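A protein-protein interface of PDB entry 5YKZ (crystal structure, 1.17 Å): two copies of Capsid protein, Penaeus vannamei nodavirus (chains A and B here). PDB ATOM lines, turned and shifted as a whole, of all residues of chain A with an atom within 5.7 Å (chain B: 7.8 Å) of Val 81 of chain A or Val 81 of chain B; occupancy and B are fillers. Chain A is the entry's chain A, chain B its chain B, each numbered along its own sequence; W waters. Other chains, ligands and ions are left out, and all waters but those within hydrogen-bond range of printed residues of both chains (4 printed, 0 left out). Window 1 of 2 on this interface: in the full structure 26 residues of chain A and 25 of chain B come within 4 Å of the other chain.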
ATOM      1  N   PRO A  43      31.594   5.579  27.236  1.00  0.00           N
ATOM      2  CA  PRO A  43      31.062   5.764  28.614  1.00  0.00           C
ATOM      3  C   PRO A  43      30.891   4.494  29.409  1.00  0.00           C
ATOM      4  O   PRO A  43      30.692   3.415  28.840  1.00  0.00           O
ATOM      5  CB  PRO A  43      29.705   6.382  28.353  1.00  0.00           C
ATOM      6  CG  PRO A  43      29.277   5.794  27.037  1.00  0.00           C
ATOM      7  CD  PRO A  43      30.525   5.707  26.221  1.00  0.00           C
ATOM      8  N   ALA A  44      30.954   4.623  30.735  1.00  0.00           N
ATOM      9  CA  ALA A  44      30.677   3.492  31.599  1.00  0.00           C
ATOM     10  C   ALA A  44      30.400   3.995  33.010  1.00  0.00           C
ATOM     11  O   ALA A  44      30.926   5.070  33.395  1.00  0.00           O
ATOM     12  CB  ALA A  44      31.841   2.572  31.668  1.00  0.00           C
ATOM     13  N   PHE A  45      29.662   3.260  33.831  1.00  0.00           N
ATOM     14  CA  PHE A  45      29.539   3.579  35.227  1.00  0.00           C
ATOM     15  C   PHE A  45      29.097   2.369  35.954  1.00  0.00           C
ATOM     16  O   PHE A  45      28.517   1.417  35.393  1.00  0.00           O
ATOM     17  CB  PHE A  45      28.564   4.768  35.474  1.00  0.00           C
ATOM     18  CG  PHE A  45      27.192   4.594  34.911  1.00  0.00           C
ATOM     19  CD1 PHE A  45      26.264   3.730  35.549  1.00  0.00           C
ATOM     20  CD2 PHE A  45      26.849   5.197  33.731  1.00  0.00           C
ATOM     21  CE1 PHE A  45      25.029   3.546  34.993  1.00  0.00           C
ATOM     22  CE2 PHE A  45      25.586   4.993  33.239  1.00  0.00           C
ATOM     23  CZ  PHE A  45      24.682   4.158  33.833  1.00  0.00           C
ATOM     24  N   LEU A  46      29.305   2.367  37.286  1.00  0.00           N
ATOM     25  CA  LEU A  46      29.176   1.176  38.108  1.00  0.00           C
ATOM     26  C   LEU A  46      28.369   1.433  39.320  1.00  0.00           C
ATOM     27  O   LEU A  46      28.732   2.243  40.167  1.00  0.00           O
ATOM     28  CB  LEU A  46      30.584   0.684  38.471  1.00  0.00           C
ATOM     29  CG  LEU A  46      30.628  -0.582  39.312  1.00  0.00           C
ATOM     30  CD1 LEU A  46      30.068  -1.792  38.545  1.00  0.00           C
ATOM     31  CD2 LEU A  46      32.055  -0.860  39.769  1.00  0.00           C
ATOM     32  N   SER A  71      26.892  10.821  25.713  1.00  0.00           N
ATOM     33  CA  SER A  71      25.660  11.163  26.359  1.00  0.00           C
ATOM     34  C   SER A  71      25.272  10.166  27.416  1.00  0.00           C
ATOM     35  O   SER A  71      25.147   8.970  27.111  1.00  0.00           O
ATOM     36  CB  SER A  71      24.549  11.156  25.278  1.00  0.00           C
ATOM     37  OG  SER A  71      24.794  12.151  24.267  1.00  0.00           O
ATOM     38  N   ILE A  72      25.067  10.634  28.614  1.00  0.00           N
ATOM     39  CA  ILE A  72      24.531   9.792  29.672  1.00  0.00           C
ATOM     40  C   ILE A  72      23.283  10.499  30.234  1.00  0.00           C
ATOM     41  O   ILE A  72      23.445  11.535  30.941  1.00  0.00           O
ATOM     42  CB  ILE A  72      25.536   9.591  30.804  1.00  0.00           C
ATOM     43  CG1 ILE A  72      26.810   8.919  30.265  1.00  0.00           C
ATOM     44  CG2 ILE A  72      24.896   8.751  31.910  1.00  0.00           C
ATOM     45  CD1 ILE A  72      27.893   8.752  31.354  1.00  0.00           C
ATOM     46  N   ASN A  73      22.119  10.037  29.895  1.00  0.00           N
ATOM     47  CA  ASN A  73      20.873  10.657  30.285  1.00  0.00           C
ATOM     48  C   ASN A  73      20.050   9.621  30.988  1.00  0.00           C
ATOM     49  O   ASN A  73      19.595   8.679  30.338  1.00  0.00           O
ATOM     50  CB  ASN A  73      20.088  11.237  29.088  1.00  0.00           C
ATOM     51  CG  ASN A  73      18.823  11.896  29.466  1.00  0.00           C
ATOM     52  OD1 ASN A  73      18.312  11.655  30.482  1.00  0.00           O
ATOM     53  ND2 ASN A  73      18.390  12.852  28.634  1.00  0.00           N
ATOM     54  N   MET A  74      19.898   9.749  32.304  1.00  0.00           N
ATOM     55  CA  MET A  74      19.260   8.738  33.113  1.00  0.00           C
ATOM     56  C   MET A  74      17.775   9.030  33.296  1.00  0.00           C
ATOM     57  O   MET A  74      17.141   8.436  34.160  1.00  0.00           O
ATOM     58  CB  MET A  74      19.993   8.567  34.453  1.00  0.00           C
ATOM     59  CG  MET A  74      21.436   8.146  34.200  1.00  0.00           C
ATOM     60  SD  MET A  74      21.762   6.879  33.017  1.00  0.00           S
ATOM     61  CE  MET A  74      20.946   5.714  33.805  1.00  0.00           C
ATOM     62  N   THR A  79      16.110   6.725  28.431  1.00  0.00           N
ATOM     63  CA  THR A  79      17.433   6.570  29.054  1.00  0.00           C
ATOM     64  C   THR A  79      18.455   6.267  27.982  1.00  0.00           C
ATOM     65  O   THR A  79      18.231   5.404  27.103  1.00  0.00           O
ATOM     66  CB  THR A  79      17.345   5.384  30.008  1.00  0.00           C
ATOM     67  OG1 THR A  79      16.171   5.464  30.858  1.00  0.00           O
ATOM     68  CG2 THR A  79      18.534   5.352  30.909  1.00  0.00           C
ATOM     69  N   THR A  80      19.593   6.950  28.030  1.00  0.00           N
ATOM     70  CA  THR A  80      20.644   6.840  27.029  1.00  0.00           C
ATOM     71  C   THR A  80      21.992   6.719  27.724  1.00  0.00           C
ATOM     72  O   THR A  80      22.313   7.557  28.590  1.00  0.00           O
ATOM     73  CB  THR A  80      20.684   8.050  26.113  1.00  0.00           C
ATOM     74  OG1 THR A  80      19.452   8.047  25.344  1.00  0.00           O
ATOM     75  CG2 THR A  80      21.829   8.085  25.186  1.00  0.00           C
ATOM     76  N   VAL A  81      22.807   5.766  27.319  1.00  0.00           N
ATOM     77  CA  VAL A  81      24.209   5.713  27.671  1.00  0.00           C
ATOM     78  C   VAL A  81      24.916   5.351  26.381  1.00  0.00           C
ATOM     79  O   VAL A  81      24.936   4.198  25.975  1.00  0.00           O
ATOM     80  CB  VAL A  81      24.480   4.685  28.755  1.00  0.00           C
ATOM     81  CG1 VAL A  81      25.956   4.698  29.129  1.00  0.00           C
ATOM     82  CG2 VAL A  81      23.711   4.985  30.010  1.00  0.00           C
ATOM     83  N   SER A  82      25.387   6.361  25.649  1.00  0.00           N
ATOM     84  CA  SER A  82      25.776   6.153  24.294  1.00  0.00           C
ATOM     85  C   SER A  82      26.739   7.208  23.793  1.00  0.00           C
ATOM     86  O   SER A  82      27.049   8.193  24.467  1.00  0.00           O
ATOM     87  CB  SER A  82      24.523   6.111  23.407  1.00  0.00           C
ATOM     88  OG  SER A  82      24.757   5.585  22.092  1.00  0.00           O
ATOM     89  N   GLY A  83      27.210   7.026  22.566  1.00  0.00           N
ATOM     90  CA  GLY A  83      28.134   7.973  21.962  1.00  0.00           C
ATOM     91  C   GLY A  83      29.561   7.538  22.297  1.00  0.00           C
ATOM     92  O   GLY A  83      29.850   6.790  23.193  1.00  0.00           O
ATOM     93  N   THR B  42      32.188  -2.601  23.957  1.00  0.00           N
ATOM     94  CA  THR B  42      31.758  -1.734  25.021  1.00  0.00           C
ATOM     95  C   THR B  42      30.261  -1.539  24.937  1.00  0.00           C
ATOM     96  O   THR B  42      29.706  -1.483  23.811  1.00  0.00           O
ATOM     97  CB  THR B  42      32.505  -0.377  24.911  1.00  0.00           C
ATOM     98  OG1 THR B  42      32.278   0.210  23.566  1.00  0.00           O
ATOM     99  CG2 THR B  42      33.945  -0.554  25.109  1.00  0.00           C
ATOM    100  N   PRO B  43      29.567  -1.416  26.053  1.00  0.00           N
ATOM    101  CA  PRO B  43      28.095  -1.334  26.032  1.00  0.00           C
ATOM    102  C   PRO B  43      27.569   0.013  25.611  1.00  0.00           C
ATOM    103  O   PRO B  43      28.228   1.031  25.876  1.00  0.00           O
ATOM    104  CB  PRO B  43      27.725  -1.606  27.509  1.00  0.00           C
ATOM    105  CG  PRO B  43      28.934  -1.100  28.273  1.00  0.00           C
ATOM    106  CD  PRO B  43      30.112  -1.459  27.442  1.00  0.00           C
ATOM    107  N   ALA B  44      26.376   0.085  25.111  1.00  0.00           N
ATOM    108  CA  ALA B  44      25.693   1.333  24.768  1.00  0.00           C
ATOM    109  C   ALA B  44      24.228   1.083  24.582  1.00  0.00           C
ATOM    110  O   ALA B  44      23.840  -0.037  24.098  1.00  0.00           O
ATOM    111  CB  ALA B  44      26.270   1.970  23.515  1.00  0.00           C
ATOM    112  N   PHE B  45      23.381   2.078  24.773  1.00  0.00           N
ATOM    113  CA  PHE B  45      21.992   1.986  24.361  1.00  0.00           C
ATOM    114  C   PHE B  45      21.446   3.401  24.235  1.00  0.00           C
ATOM    115  O   PHE B  45      22.002   4.364  24.811  1.00  0.00           O
ATOM    116  CB  PHE B  45      21.152   1.123  25.296  1.00  0.00           C
ATOM    117  CG  PHE B  45      21.164   1.599  26.717  1.00  0.00           C
ATOM    118  CD1 PHE B  45      20.444   2.675  27.122  1.00  0.00           C
ATOM    119  CD2 PHE B  45      21.931   0.941  27.640  1.00  0.00           C
ATOM    120  CE1 PHE B  45      20.509   3.101  28.483  1.00  0.00           C
ATOM    121  CE2 PHE B  45      21.997   1.354  28.927  1.00  0.00           C
ATOM    122  CZ  PHE B  45      21.288   2.434  29.331  1.00  0.00           C
ATOM    123  N   LEU B  46      20.363   3.559  23.492  1.00  0.00           N
ATOM    124  CA  LEU B  46      19.856   4.846  23.100  1.00  0.00           C
ATOM    125  C   LEU B  46      18.371   4.965  23.341  1.00  0.00           C
ATOM    126  O   LEU B  46      17.590   4.177  22.762  1.00  0.00           O
ATOM    127  CB  LEU B  46      20.197   5.076  21.608  1.00  0.00           C
ATOM    128  CG  LEU B  46      19.794   6.378  21.056  1.00  0.00           C
ATOM    129  CD1 LEU B  46      20.432   7.585  21.702  1.00  0.00           C
ATOM    130  CD2 LEU B  46      20.118   6.472  19.587  1.00  0.00           C
ATOM    131  N   GLU B  47      17.968   5.948  24.088  1.00  0.00           N
ATOM    132  CA  GLU B  47      16.565   6.346  24.173  1.00  0.00           C
ATOM    133  C   GLU B  47      15.668   5.191  24.523  1.00  0.00           C
ATOM    134  O   GLU B  47      14.617   4.977  23.849  1.00  0.00           O
ATOM    135  CB  GLU B  47      16.135   7.105  22.939  1.00  0.00           C
ATOM    136  CG  GLU B  47      16.912   8.404  22.756  1.00  0.00           C
ATOM    137  CD  GLU B  47      16.877   9.029  21.390  1.00  0.00           C
ATOM    138  OE1 GLU B  47      17.516  10.129  21.265  1.00  0.00           O
ATOM    139  OE2 GLU B  47      16.379   8.414  20.430  1.00  0.00           O
ATOM    140  N   GLN B  48      15.952   4.461  25.591  1.00  0.00           N
ATOM    141  CA  GLN B  48      15.150   3.302  26.055  1.00  0.00           C
ATOM    142  C   GLN B  48      14.292   3.637  27.162  1.00  0.00           C
ATOM    143  O   GLN B  48      14.666   4.359  28.081  1.00  0.00           O
ATOM    144  CB  GLN B  48      16.091   2.117  26.411  1.00  0.00           C
ATOM    145  CG  GLN B  48      16.854   1.605  25.236  1.00  0.00           C
ATOM    146  CD  GLN B  48      15.980   1.102  24.160  1.00  0.00           C
ATOM    147  OE1 GLN B  48      15.190   0.176  24.436  1.00  0.00           O
ATOM    148  NE2 GLN B  48      16.110   1.608  23.017  1.00  0.00           N
ATOM    149  N   PHE B  50      13.057   1.660  30.008  1.00  0.00           N
ATOM    150  CA  PHE B  50      13.167   0.417  30.779  1.00  0.00           C
ATOM    151  C   PHE B  50      12.053   0.285  31.765  1.00  0.00           C
ATOM    152  O   PHE B  50      12.038  -0.757  32.433  1.00  0.00           O
ATOM    153  CB  PHE B  50      14.550   0.362  31.493  1.00  0.00           C
ATOM    154  CG  PHE B  50      15.717   0.338  30.574  1.00  0.00           C
ATOM    155  CD1 PHE B  50      16.060  -0.834  29.869  1.00  0.00           C
ATOM    156  CD2 PHE B  50      16.548   1.420  30.381  1.00  0.00           C
ATOM    157  CE1 PHE B  50      17.143  -0.872  29.080  1.00  0.00           C
ATOM    158  CE2 PHE B  50      17.646   1.389  29.582  1.00  0.00           C
ATOM    159  CZ  PHE B  50      17.935   0.218  28.905  1.00  0.00           C
ATOM    160  N   ILE B  70      30.269  -7.763  29.984  1.00  0.00           N
ATOM    161  CA  ILE B  70      29.427  -6.536  29.931  1.00  0.00           C
ATOM    162  C   ILE B  70      28.249  -6.723  30.829  1.00  0.00           C
ATOM    163  O   ILE B  70      27.572  -7.755  30.772  1.00  0.00           O
ATOM    164  CB  ILE B  70      29.033  -6.217  28.468  1.00  0.00           C
ATOM    165  CG1 ILE B  70      30.223  -5.648  27.777  1.00  0.00           C
ATOM    166  CG2 ILE B  70      27.894  -5.263  28.467  1.00  0.00           C
ATOM    167  CD1 ILE B  70      30.011  -5.404  26.269  1.00  0.00           C
ATOM    168  N   SER B  71      28.011  -5.709  31.669  1.00  0.00           N
ATOM    169  CA  SER B  71      26.895  -5.693  32.563  1.00  0.00           C
ATOM    170  C   SER B  71      26.033  -4.472  32.297  1.00  0.00           C
ATOM    171  O   SER B  71      26.543  -3.326  32.316  1.00  0.00           O
ATOM    172  CB  SER B  71      27.359  -5.625  34.015  1.00  0.00           C
ATOM    173  OG  SER B  71      26.289  -5.348  34.864  1.00  0.00           O
ATOM    174  N   ILE B  72      24.753  -4.686  32.044  1.00  0.00           N
ATOM    175  CA  ILE B  72      23.760  -3.608  31.944  1.00  0.00           C
ATOM    176  C   ILE B  72      22.676  -3.954  32.922  1.00  0.00           C
ATOM    177  O   ILE B  72      21.820  -4.826  32.653  1.00  0.00           O
ATOM    178  CB  ILE B  72      23.197  -3.440  30.498  1.00  0.00           C
ATOM    179  CG1 ILE B  72      24.296  -3.125  29.508  1.00  0.00           C
ATOM    180  CG2 ILE B  72      22.131  -2.404  30.530  1.00  0.00           C
ATOM    181  CD1 ILE B  72      23.908  -3.031  28.079  1.00  0.00           C
ATOM    182  N   ASN B  73      22.645  -3.319  34.063  1.00  0.00           N
ATOM    183  CA  ASN B  73      21.693  -3.551  35.149  1.00  0.00           C
ATOM    184  C   ASN B  73      20.992  -2.223  35.384  1.00  0.00           C
ATOM    185  O   ASN B  73      21.607  -1.271  35.893  1.00  0.00           O
ATOM    186  CB  ASN B  73      22.344  -4.134  36.391  1.00  0.00           C
ATOM    187  CG  ASN B  73      21.307  -4.378  37.465  1.00  0.00           C
ATOM    188  OD1 ASN B  73      20.307  -3.824  37.509  1.00  0.00           O
ATOM    189  ND2 ASN B  73      21.673  -5.304  38.380  1.00  0.00           N
ATOM    190  N   MET B  74      19.736  -2.128  35.000  1.00  0.00           N
ATOM    191  CA  MET B  74      18.986  -0.931  35.088  1.00  0.00           C
ATOM    192  C   MET B  74      18.241  -0.781  36.460  1.00  0.00           C
ATOM    193  O   MET B  74      17.349   0.027  36.580  1.00  0.00           O
ATOM    194  CB  MET B  74      18.091  -0.731  33.903  1.00  0.00           C
ATOM    195  CG  MET B  74      18.877  -0.648  32.594  1.00  0.00           C
ATOM    196  SD  MET B  74      20.323   0.357  32.554  1.00  0.00           S
ATOM    197  CE  MET B  74      19.596   1.771  32.762  1.00  0.00           C
ATOM    198  N   VAL B  78      20.849   0.659  41.859  1.00  0.00           N
ATOM    199  CA  VAL B  78      22.160   0.183  41.678  1.00  0.00           C
ATOM    200  C   VAL B  78      22.311  -0.037  40.188  1.00  0.00           C
ATOM    201  O   VAL B  78      22.185  -1.178  39.671  1.00  0.00           O
ATOM    202  CB  VAL B  78      22.540  -1.026  42.563  1.00  0.00           C
ATOM    203  CG1 VAL B  78      21.574  -2.209  42.413  1.00  0.00           C
ATOM    204  CG2 VAL B  78      23.983  -1.397  42.395  1.00  0.00           C
ATOM    205  N   THR B  79      22.497   1.052  39.473  1.00  0.00           N
ATOM    206  CA  THR B  79      22.478   1.005  37.960  1.00  0.00           C
ATOM    207  C   THR B  79      23.874   0.879  37.458  1.00  0.00           C
ATOM    208  O   THR B  79      24.783   1.650  37.863  1.00  0.00           O
ATOM    209  CB  THR B  79      21.876   2.289  37.463  1.00  0.00           C
ATOM    210  OG1 THR B  79      20.645   2.602  38.121  1.00  0.00           O
ATOM    211  CG2 THR B  79      21.607   2.176  35.992  1.00  0.00           C
ATOM    212  N   THR B  80      24.125  -0.104  36.600  1.00  0.00           N
ATOM    213  CA  THR B  80      25.448  -0.351  36.020  1.00  0.00           C
ATOM    214  C   THR B  80      25.364  -0.418  34.511  1.00  0.00           C
ATOM    215  O   THR B  80      24.483  -1.153  33.988  1.00  0.00           O
ATOM    216  CB  THR B  80      26.003  -1.650  36.561  1.00  0.00           C
ATOM    217  OG1 THR B  80      26.218  -1.514  37.968  1.00  0.00           O
ATOM    218  CG2 THR B  80      27.270  -2.091  35.923  1.00  0.00           C
ATOM    219  N   VAL B  81      26.241   0.282  33.836  1.00  0.00           N
ATOM    220  CA  VAL B  81      26.460   0.088  32.375  1.00  0.00           C
ATOM    221  C   VAL B  81      27.955   0.041  32.255  1.00  0.00           C
ATOM    222  O   VAL B  81      28.602   1.110  32.201  1.00  0.00           O
ATOM    223  CB  VAL B  81      25.810   1.168  31.572  1.00  0.00           C
ATOM    224  CG1 VAL B  81      26.041   0.915  30.085  1.00  0.00           C
ATOM    225  CG2 VAL B  81      24.292   1.250  31.811  1.00  0.00           C
ATOM    226  N   SER B  82      28.553  -1.151  32.301  1.00  0.00           N
ATOM    227  CA  SER B  82      29.993  -1.204  32.491  1.00  0.00           C
ATOM    228  C   SER B  82      30.545  -2.517  31.941  1.00  0.00           C
ATOM    229  O   SER B  82      29.782  -3.433  31.521  1.00  0.00           O
ATOM    230  CB  SER B  82      30.293  -1.081  33.959  1.00  0.00           C
ATOM    231  OG  SER B  82      31.666  -0.692  34.131  1.00  0.00           O
ATOM    232  N   GLY B  83      31.846  -2.621  31.987  1.00  0.00           N
ATOM    233  CA  GLY B  83      32.563  -3.756  31.445  1.00  0.00           C
ATOM    234  C   GLY B  83      32.924  -3.621  30.022  1.00  0.00           C
ATOM    235  O   GLY B  83      32.256  -2.920  29.276  1.00  0.00           O
ATOM    236  N   THR B 110      19.351  -2.966  23.815  1.00  0.00           N
ATOM    237  CA  THR B 110      20.687  -2.476  24.204  1.00  0.00           C
ATOM    238  C   THR B 110      21.664  -3.144  23.251  1.00  0.00           C
ATOM    239  O   THR B 110      21.312  -4.019  22.464  1.00  0.00           O
ATOM    240  CB  THR B 110      21.012  -2.741  25.648  1.00  0.00           C
ATOM    241  OG1 THR B 110      21.250  -4.120  25.865  1.00  0.00           O
ATOM    242  CG2 THR B 110      19.932  -2.219  26.580  1.00  0.00           C
ATOM    243  N   GLY B 111      22.937  -2.748  23.341  1.00  0.00           N
ATOM    244  CA  GLY B 111      23.927  -3.247  22.431  1.00  0.00           C
ATOM    245  C   GLY B 111      25.330  -2.907  22.839  1.00  0.00           C
ATOM    246  O   GLY B 111      25.613  -2.569  24.007  1.00  0.00           O
ATOM    247  N   ASN B 113      29.372  -1.568  21.038  1.00  0.00           N
ATOM    248  CA  ASN B 113      30.277  -1.163  19.984  1.00  0.00           C
ATOM    249  C   ASN B 113      31.356  -2.108  19.807  1.00  0.00           C
ATOM    250  O   ASN B 113      31.882  -2.595  20.799  1.00  0.00           O
ATOM    251  CB  ASN B 113      30.819   0.243  20.275  1.00  0.00           C
ATOM    252  CG  ASN B 113      29.664   1.304  19.980  1.00  0.00           C
ATOM    253  OD1 ASN B 113      29.005   1.255  18.976  1.00  0.00           O
ATOM    254  ND2 ASN B 113      29.395   1.995  20.855  1.00  0.00           N
HETATM  255  O   HOH W   1      23.453   3.195  21.463  1.00  0.00           O
HETATM  256  O   HOH W   2      30.485   2.136  26.285  1.00  0.00           O
HETATM  257  O   HOH W   3      14.175   3.789  31.535  1.00  0.00           O
HETATM  258  O   HOH W   4      27.382   4.304  20.916  1.00  0.00           O
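The backbone NH (N) of Phe 45 of chain A lies within hydrogen-bond range of the backbone carbonyl oxygen (O) of Val 81 of chain B (2.9 Å). N of Glu 47 of chain B sits at hydrogen-bond distance from O of Thr 79 of chain A. O of Gln 48 of chain B lies within hydrogen-bond range of N of Thr 79 of chain A, 2.8 Å away. OG1 of Thr 80 of chain A sits at hydrogen-bond distance from N of Glu 47 of chain B (2.9 Å). N of Phe 45 of chain B lies within hydrogen-bond range of O of Val 81 of chain A (2.9 Å).
N of Ser 71 of chain A is in hydrogen-bond range of O of Ser 82 of chain A (2.9 Å). The backbone NH (N) of Asn 73 of chain A sits at hydrogen-bond distance from the backbone carbonyl oxygen (O) of Thr 80 of chain A, at 2.8 Å. O of Ala 44 of chain B lies within hydrogen-bond range of N of Gly 111 of chain B, 3.0 Å away. The side-chain amide nitrogen (NE2) of Gln 48 of chain B lies within hydrogen-bond range of the backbone carbonyl oxygen (O) of Leu 46 of chain B (3.0 Å). The backbone NH of Ser 71 of chain B sits at hydrogen-bond distance from the backbone carbonyl oxygen of Ser 82 of chain B (2.9 Å). The backbone NH (N) of Asn 73 of chain B sits at hydrogen-bond distance from the backbone carbonyl oxygen (O) of Thr 80 of chain B (2.8 Å).
Among the printed residues, pairs that only touch across the chains: Val 81 of chain A with Ala 44 of chain B, Ala 44 of chain A with Val 81 of chain B, Ser 82 of chain A with Phe 45 of chain B, Phe 45 of chain A with Ser 82 of chain B, Phe 45 of chain A with Thr 79 of chain B, Thr 79 of chain A with Phe 45 of chain B, Thr 80 of chain A with Phe 45 of chain B, Phe 45 of chain A with Thr 80 of chain B, Thr 80 of chain A with Leu 46 of chain B, Thr 79 of chain A with Leu 46 of chain B, Leu 46 of chain A with Thr 80 of chain B, Leu 46 of chain A with Thr 79 of chain B and Val 81 of chain A with Val 81 of chain B.
Of the printed residues of chain B, Val 81 of chain A touches Ala 44 (3.2 Å), Phe 45 (2.9 Å) and Val 81 (3.9 Å). Printed residues of chain A within 4 Å of Val 81 of chain B: Ala 44 (3.2 Å), Phe 45 (2.9 Å) and Val 81 (3.9 Å). Of the printed residues of chain B, Leu 46 of chain A touches Thr 79 and Thr 80. Of the printed residues of chain A, Glu 47 of chain B touches Thr 79 (3.1 Å) and Thr 80 (2.9 Å). Printed residues of chain A within 4 Å of Phe 45 of chain B: Thr 79, Thr 80, Val 81 and Ser 82. Met 74 of chain A touches none of the printed residues of chain B. Gly 83 of chain B touches none of the printed residues of chain A. The nearest residue of chain B that does not touch Val 81 of chain A is Pro 43 of chain B (4.6 Å). The nearest printed residue of chain B that does not touch Ala 44 of chain A is Ser 82 of chain B (4.1 Å).
Hydrophobic or aromatic side chains of chain B that line the printed part of chain A: Ala 44, Phe 45, Leu 46 and Val 81. Hydrophobic or aromatic side chains of chain A within 4 Å of the printed part of chain B: Ala 44, Phe 45, Leu 46 and Val 81. Among the printed residues, 18 pairs touch across the chains. Among the printed residues, no Asp or Glu carboxylate lies within 4 Å of a Lys or Arg side-chain nitrogen of the other chain.
Ala 44 of chain A touches Val 81 of chain B, and with the chains exchanged Val 81 of chain A touches Ala 44 of chain B. Phe 45 of chain A touches Thr 80 of chain B, and with the chains exchanged Thr 80 of chain A touches Phe 45 of chain B. Phe 45 of chain A touches Ser 82 of chain B, and with the chains exchanged Ser 82 of chain A touches Phe 45 of chain B. Val 81 of chain A touches its own counterpart, Val 81 of chain B. Of the 18 pairs that touch across the chains among the printed residues, 15 have their exchanged pair printed and touching as well.
Water W2 bridges the backbone carbonyl oxygen of Pro 43 of chain B and the backbone carbonyl oxygen of Pro 43 of chain A. Water W3 lies within hydrogen-bond range of OG1 of Thr 79 of chain A (2.7 Å) and N of Phe 50 of chain B (2.8 Å). Water W1 lies within hydrogen-bond range of the side-chain hydroxyl of Ser 82 of chain A (2.8 Å) and the backbone NH of Phe 45 of chain B (3.5 Å). Water W4 lies within hydrogen-bond range of the side-chain amide nitrogen (ND2) of Asn 113 of chain B (3.1 Å), the side-chain hydroxyl (OG) of Ser 82 of chain A (3.1 Å) and the backbone NH (N) of Gly 83 of chain A (3.2 Å).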
